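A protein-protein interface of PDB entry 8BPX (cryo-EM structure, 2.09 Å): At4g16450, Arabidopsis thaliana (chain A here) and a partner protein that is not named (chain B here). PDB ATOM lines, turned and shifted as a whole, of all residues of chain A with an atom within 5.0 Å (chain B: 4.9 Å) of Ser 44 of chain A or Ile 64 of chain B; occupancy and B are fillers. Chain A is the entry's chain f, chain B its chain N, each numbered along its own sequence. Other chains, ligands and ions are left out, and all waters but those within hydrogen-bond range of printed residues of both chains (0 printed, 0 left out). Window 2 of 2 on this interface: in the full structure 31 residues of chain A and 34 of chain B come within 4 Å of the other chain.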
ATOM      1  N   THR A  39      -4.373   5.094  24.510  1.00  0.00           N
ATOM      2  CA  THR A  39      -4.154   5.711  25.813  1.00  0.00           C
ATOM      3  C   THR A  39      -4.260   7.227  25.728  1.00  0.00           C
ATOM      4  O   THR A  39      -4.917   7.863  26.563  1.00  0.00           O
ATOM      5  CB  THR A  39      -2.785   5.305  26.368  1.00  0.00           C
ATOM      6  OG1 THR A  39      -2.738   3.886  26.548  1.00  0.00           O
ATOM      7  CG2 THR A  39      -2.518   5.994  27.698  1.00  0.00           C
ATOM      8  N   ILE A  40      -3.611   7.825  24.727  1.00  0.00           N
ATOM      9  CA  ILE A  40      -3.646   9.279  24.600  1.00  0.00           C
ATOM     10  C   ILE A  40      -5.075   9.750  24.355  1.00  0.00           C
ATOM     11  O   ILE A  40      -5.555  10.698  24.996  1.00  0.00           O
ATOM     12  CB  ILE A  40      -2.678   9.739  23.494  1.00  0.00           C
ATOM     13  CG1 ILE A  40      -1.234   9.659  24.000  1.00  0.00           C
ATOM     14  CG2 ILE A  40      -2.989  11.161  23.049  1.00  0.00           C
ATOM     15  CD1 ILE A  40      -0.207   9.470  22.910  1.00  0.00           C
ATOM     16  N   THR A  41      -5.797   9.063  23.462  1.00  0.00           N
ATOM     17  CA  THR A  41      -7.184   9.438  23.198  1.00  0.00           C
ATOM     18  C   THR A  41      -8.062   9.292  24.439  1.00  0.00           C
ATOM     19  O   THR A  41      -8.898  10.161  24.719  1.00  0.00           O
ATOM     20  CB  THR A  41      -7.740   8.605  22.046  1.00  0.00           C
ATOM     21  OG1 THR A  41      -6.820   8.637  20.947  1.00  0.00           O
ATOM     22  CG2 THR A  41      -9.100   9.135  21.607  1.00  0.00           C
ATOM     23  N   GLY A  42      -7.898   8.200  25.190  1.00  0.00           N
ATOM     24  CA  GLY A  42      -8.725   7.989  26.367  1.00  0.00           C
ATOM     25  C   GLY A  42      -8.475   9.019  27.450  1.00  0.00           C
ATOM     26  O   GLY A  42      -9.420   9.540  28.052  1.00  0.00           O
ATOM     27  N   ILE A  43      -7.203   9.328  27.712  1.00  0.00           N
ATOM     28  CA  ILE A  43      -6.877  10.376  28.674  1.00  0.00           C
ATOM     29  C   ILE A  43      -7.487  11.701  28.237  1.00  0.00           C
ATOM     30  O   ILE A  43      -8.030  12.454  29.057  1.00  0.00           O
ATOM     31  CB  ILE A  43      -5.352  10.486  28.849  1.00  0.00           C
ATOM     32  CG1 ILE A  43      -4.800   9.270  29.594  1.00  0.00           C
ATOM     33  CG2 ILE A  43      -4.979  11.770  29.581  1.00  0.00           C
ATOM     34  CD1 ILE A  43      -3.298   9.152  29.503  1.00  0.00           C
ATOM     35  N   SER A  44      -7.399  12.011  26.942  1.00  0.00           N
ATOM     36  CA  SER A  44      -7.930  13.280  26.460  1.00  0.00           C
ATOM     37  C   SER A  44      -9.445  13.354  26.621  1.00  0.00           C
ATOM     38  O   SER A  44      -9.980  14.392  27.028  1.00  0.00           O
ATOM     39  CB  SER A  44      -7.520  13.490  25.008  1.00  0.00           C
ATOM     40  OG  SER A  44      -6.122  13.690  24.908  1.00  0.00           O
ATOM     41  N   VAL A  45     -10.151  12.260  26.318  1.00  0.00           N
ATOM     42  CA  VAL A  45     -11.601  12.237  26.504  1.00  0.00           C
ATOM     43  C   VAL A  45     -11.951  12.408  27.978  1.00  0.00           C
ATOM     44  O   VAL A  45     -12.900  13.122  28.329  1.00  0.00           O
ATOM     45  CB  VAL A  45     -12.205  10.941  25.930  1.00  0.00           C
ATOM     46  CG1 VAL A  45     -13.680  10.840  26.284  1.00  0.00           C
ATOM     47  CG2 VAL A  45     -12.022  10.883  24.424  1.00  0.00           C
ATOM     48  N   THR A  46     -11.197  11.748  28.862  1.00  0.00           N
ATOM     49  CA  THR A  46     -11.452  11.862  30.294  1.00  0.00           C
ATOM     50  C   THR A  46     -11.274  13.299  30.775  1.00  0.00           C
ATOM     51  O   THR A  46     -12.096  13.818  31.541  1.00  0.00           O
ATOM     52  CB  THR A  46     -10.525  10.917  31.062  1.00  0.00           C
ATOM     53  OG1 THR A  46     -10.886   9.558  30.781  1.00  0.00           O
ATOM     54  CG2 THR A  46     -10.619  11.166  32.562  1.00  0.00           C
ATOM     55  N   VAL A  47     -10.195  13.953  30.336  1.00  0.00           N
ATOM     56  CA  VAL A  47      -9.961  15.344  30.714  1.00  0.00           C
ATOM     57  C   VAL A  47     -11.081  16.231  30.187  1.00  0.00           C
ATOM     58  O   VAL A  47     -11.575  17.116  30.894  1.00  0.00           O
ATOM     59  CB  VAL A  47      -8.576  15.815  30.224  1.00  0.00           C
ATOM     60  CG1 VAL A  47      -8.411  17.313  30.439  1.00  0.00           C
ATOM     61  CG2 VAL A  47      -7.469  15.060  30.944  1.00  0.00           C
ATOM     62  N   GLY A  48     -11.505  15.998  28.942  1.00  0.00           N
ATOM     63  CA  GLY A  48     -12.619  16.759  28.402  1.00  0.00           C
ATOM     64  C   GLY A  48     -13.875  16.618  29.240  1.00  0.00           C
ATOM     65  O   GLY A  48     -14.522  17.609  29.580  1.00  0.00           O
ATOM     66  N   GLY A  65     -12.015  17.304  23.618  1.00  0.00           N
ATOM     67  CA  GLY A  65     -10.859  16.600  24.139  1.00  0.00           C
ATOM     68  C   GLY A  65     -10.520  15.370  23.324  1.00  0.00           C
ATOM     69  O   GLY A  65      -9.349  15.083  23.080  1.00  0.00           O
ATOM     70  N   GLY A  66     -11.543  14.643  22.871  1.00  0.00           N
ATOM     71  CA  GLY A  66     -11.306  13.465  22.063  1.00  0.00           C
ATOM     72  C   GLY A  66     -10.711  13.785  20.708  1.00  0.00           C
ATOM     73  O   GLY A  66      -9.892  13.026  20.194  1.00  0.00           O
ATOM     74  N   ILE A  68      -8.734  16.396  20.088  1.00  0.00           N
ATOM     75  CA  ILE A  68      -7.341  16.728  20.377  1.00  0.00           C
ATOM     76  C   ILE A  68      -6.534  15.457  20.621  1.00  0.00           C
ATOM     77  O   ILE A  68      -5.424  15.292  20.096  1.00  0.00           O
ATOM     78  CB  ILE A  68      -7.258  17.693  21.572  1.00  0.00           C
ATOM     79  CG1 ILE A  68      -7.837  19.062  21.197  1.00  0.00           C
ATOM     80  CG2 ILE A  68      -5.826  17.819  22.066  1.00  0.00           C
ATOM     81  CD1 ILE A  68      -7.934  20.023  22.359  1.00  0.00           C
ATOM     82  N   GLY A  69      -7.087  14.536  21.411  1.00  0.00           N
ATOM     83  CA  GLY A  69      -6.389  13.300  21.705  1.00  0.00           C
ATOM     84  C   GLY A  69      -6.224  12.402  20.496  1.00  0.00           C
ATOM     85  O   GLY A  69      -5.190  11.761  20.334  1.00  0.00           O
ATOM     86  N   GLY A  72      -3.412  14.024  18.383  1.00  0.00           N
ATOM     87  CA  GLY A  72      -2.121  13.843  19.030  1.00  0.00           C
ATOM     88  C   GLY A  72      -1.660  12.397  19.055  1.00  0.00           C
ATOM     89  O   GLY A  72      -0.495  12.102  18.779  1.00  0.00           O
ATOM     90  N   PHE B  24       0.969  20.201  15.798  1.00  0.00           N
ATOM     91  CA  PHE B  24      -0.014  19.743  16.770  1.00  0.00           C
ATOM     92  C   PHE B  24      -0.501  20.886  17.648  1.00  0.00           C
ATOM     93  O   PHE B  24      -1.707  21.041  17.861  1.00  0.00           O
ATOM     94  CB  PHE B  24       0.545  18.631  17.654  1.00  0.00           C
ATOM     95  CG  PHE B  24      -0.365  18.292  18.799  1.00  0.00           C
ATOM     96  CD1 PHE B  24      -1.509  17.542  18.588  1.00  0.00           C
ATOM     97  CD2 PHE B  24      -0.122  18.790  20.066  1.00  0.00           C
ATOM     98  CE1 PHE B  24      -2.371  17.256  19.634  1.00  0.00           C
ATOM     99  CE2 PHE B  24      -0.982  18.513  21.109  1.00  0.00           C
ATOM    100  CZ  PHE B  24      -2.107  17.743  20.892  1.00  0.00           C
ATOM    101  N   LEU B  57      -7.993  21.804  28.860  1.00  0.00           N
ATOM    102  CA  LEU B  57      -7.728  21.227  27.545  1.00  0.00           C
ATOM    103  C   LEU B  57      -6.407  21.734  26.960  1.00  0.00           C
ATOM    104  O   LEU B  57      -5.687  20.978  26.301  1.00  0.00           O
ATOM    105  CB  LEU B  57      -8.898  21.516  26.607  1.00  0.00           C
ATOM    106  CG  LEU B  57     -10.177  20.706  26.861  1.00  0.00           C
ATOM    107  CD1 LEU B  57     -11.326  21.194  25.992  1.00  0.00           C
ATOM    108  CD2 LEU B  57      -9.941  19.218  26.654  1.00  0.00           C
ATOM    109  N   LEU B  60      -3.536  19.995  28.657  1.00  0.00           N
ATOM    110  CA  LEU B  60      -3.428  18.708  27.974  1.00  0.00           C
ATOM    111  C   LEU B  60      -2.681  18.845  26.651  1.00  0.00           C
ATOM    112  O   LEU B  60      -1.809  18.030  26.323  1.00  0.00           O
ATOM    113  CB  LEU B  60      -4.827  18.133  27.749  1.00  0.00           C
ATOM    114  CG  LEU B  60      -4.965  16.870  26.899  1.00  0.00           C
ATOM    115  CD1 LEU B  60      -4.672  15.631  27.728  1.00  0.00           C
ATOM    116  CD2 LEU B  60      -6.351  16.790  26.276  1.00  0.00           C
ATOM    117  N   SER B  61      -3.023  19.875  25.871  1.00  0.00           N
ATOM    118  CA  SER B  61      -2.381  20.078  24.574  1.00  0.00           C
ATOM    119  C   SER B  61      -0.890  20.354  24.726  1.00  0.00           C
ATOM    120  O   SER B  61      -0.074  19.838  23.953  1.00  0.00           O
ATOM    121  CB  SER B  61      -3.064  21.225  23.828  1.00  0.00           C
ATOM    122  OG  SER B  61      -4.442  20.964  23.651  1.00  0.00           O
ATOM    123  N   VAL B  62      -0.517  21.168  25.714  1.00  0.00           N
ATOM    124  CA  VAL B  62       0.893  21.450  25.971  1.00  0.00           C
ATOM    125  C   VAL B  62       1.632  20.170  26.341  1.00  0.00           C
ATOM    126  O   VAL B  62       2.754  19.928  25.879  1.00  0.00           O
ATOM    127  CB  VAL B  62       1.036  22.526  27.067  1.00  0.00           C
ATOM    128  CG1 VAL B  62       2.492  22.679  27.494  1.00  0.00           C
ATOM    129  CG2 VAL B  62       0.491  23.859  26.583  1.00  0.00           C
ATOM    130  N   LEU B  63       1.018  19.328  27.178  1.00  0.00           N
ATOM    131  CA  LEU B  63       1.685  18.094  27.584  1.00  0.00           C
ATOM    132  C   LEU B  63       1.846  17.128  26.412  1.00  0.00           C
ATOM    133  O   LEU B  63       2.880  16.459  26.291  1.00  0.00           O
ATOM    134  CB  LEU B  63       0.927  17.439  28.738  1.00  0.00           C
ATOM    135  CG  LEU B  63       0.935  18.260  30.030  1.00  0.00           C
ATOM    136  CD1 LEU B  63       0.126  17.579  31.128  1.00  0.00           C
ATOM    137  CD2 LEU B  63       2.364  18.548  30.496  1.00  0.00           C
ATOM    138  N   ILE B  64       0.847  17.055  25.530  1.00  0.00           N
ATOM    139  CA  ILE B  64       0.973  16.207  24.345  1.00  0.00           C
ATOM    140  C   ILE B  64       2.049  16.750  23.407  1.00  0.00           C
ATOM    141  O   ILE B  64       2.805  15.982  22.800  1.00  0.00           O
ATOM    142  CB  ILE B  64      -0.380  16.062  23.627  1.00  0.00           C
ATOM    143  CG1 ILE B  64      -1.387  15.331  24.519  1.00  0.00           C
ATOM    144  CG2 ILE B  64      -0.215  15.309  22.316  1.00  0.00           C
ATOM    145  CD1 ILE B  64      -2.799  15.316  23.958  1.00  0.00           C
ATOM    146  N   THR B  65       2.127  18.076  23.262  1.00  0.00           N
ATOM    147  CA  THR B  65       3.206  18.674  22.482  1.00  0.00           C
ATOM    148  C   THR B  65       4.566  18.302  23.059  1.00  0.00           C
ATOM    149  O   THR B  65       5.494  17.958  22.316  1.00  0.00           O
ATOM    150  CB  THR B  65       3.054  20.197  22.442  1.00  0.00           C
ATOM    151  OG1 THR B  65       1.744  20.546  21.974  1.00  0.00           O
ATOM    152  CG2 THR B  65       4.108  20.821  21.535  1.00  0.00           C
ATOM    153  N   LEU B  66       4.698  18.372  24.385  1.00  0.00           N
ATOM    154  CA  LEU B  66       5.947  17.995  25.035  1.00  0.00           C
ATOM    155  C   LEU B  66       6.285  16.537  24.757  1.00  0.00           C
ATOM    156  O   LEU B  66       7.441  16.207  24.474  1.00  0.00           O
ATOM    157  CB  LEU B  66       5.853  18.278  26.541  1.00  0.00           C
ATOM    158  CG  LEU B  66       6.984  18.042  27.560  1.00  0.00           C
ATOM    159  CD1 LEU B  66       7.405  16.590  27.708  1.00  0.00           C
ATOM    160  CD2 LEU B  66       8.192  18.887  27.191  1.00  0.00           C
ATOM    161  N   LEU B  67       5.293  15.650  24.844  1.00  0.00           N
ATOM    162  CA  LEU B  67       5.527  14.242  24.533  1.00  0.00           C
ATOM    163  C   LEU B  67       6.023  14.072  23.101  1.00  0.00           C
ATOM    164  O   LEU B  67       7.043  13.412  22.856  1.00  0.00           O
ATOM    165  CB  LEU B  67       4.246  13.440  24.753  1.00  0.00           C
ATOM    166  CG  LEU B  67       4.234  11.986  24.277  1.00  0.00           C
ATOM    167  CD1 LEU B  67       5.426  11.206  24.812  1.00  0.00           C
ATOM    168  CD2 LEU B  67       2.923  11.311  24.661  1.00  0.00           C
ATOM    169  N   LEU B  68       5.321  14.688  22.145  1.00  0.00           N
ATOM    170  CA  LEU B  68       5.703  14.585  20.740  1.00  0.00           C
ATOM    171  C   LEU B  68       7.126  15.077  20.515  1.00  0.00           C
ATOM    172  O   LEU B  68       7.888  14.472  19.754  1.00  0.00           O
ATOM    173  CB  LEU B  68       4.724  15.380  19.871  1.00  0.00           C
ATOM    174  CG  LEU B  68       3.366  14.747  19.550  1.00  0.00           C
ATOM    175  CD1 LEU B  68       2.462  15.751  18.844  1.00  0.00           C
ATOM    176  CD2 LEU B  68       3.545  13.504  18.704  1.00  0.00           C
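OG of Ser 44 of chain A is in hydrogen-bond range of O of Ile 40 of chain A (3.0 Å).
The side-chain hydroxyl (OG) of Ser 61 of chain B sits at hydrogen-bond distance from the backbone carbonyl oxygen (O) of Leu 57 of chain B (2.9 Å).
The backbone carbonyl oxygen (O) of Ser 61 of chain B is in hydrogen-bond range of the side-chain hydroxyl (OG1) of Thr 65 of chain B.
OG of Ser 44 of chain A touches CD2 of Leu 60 of chain B, 3.4 Å away.
Ser 44 of chain A touches Ile 64 of chain B (OG to CD1, 3.8 Å).
Gly 65 of chain A touches Leu 57 of chain B.
Phe 24 of chain B touches Ile 68 of chain A.
Ser 61 of chain B touches Ile 68 of chain A.
Phe 24 of chain B touches Gly 72 of chain A.
Ser 44 of chain A touches two residues of chain B.
Of chain A, only Ser 44 comes within 4 Å of Ile 64 of chain B.
Of the printed residues of chain B, Ile 68 of chain A touches Phe 24 and Ser 61.
Printed residues of chain A within 4 Å of Leu 57 of chain B: Gly 65.
Gly 69 of chain A touches none of the printed residues of chain B.
Hydrophobic or aromatic side chains of chain A that line the printed part of chain B: Ile 68.
Of the 11 printed residues of chain B, 5 touch a printed residue of chain A.
Hydrophobic or aromatic side chains of chain B within 4 Å of the printed part of chain A: Phe 24, Leu 57, Leu 60 and Ile 64.
Among the printed residues, 6 pairs touch across the chains.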
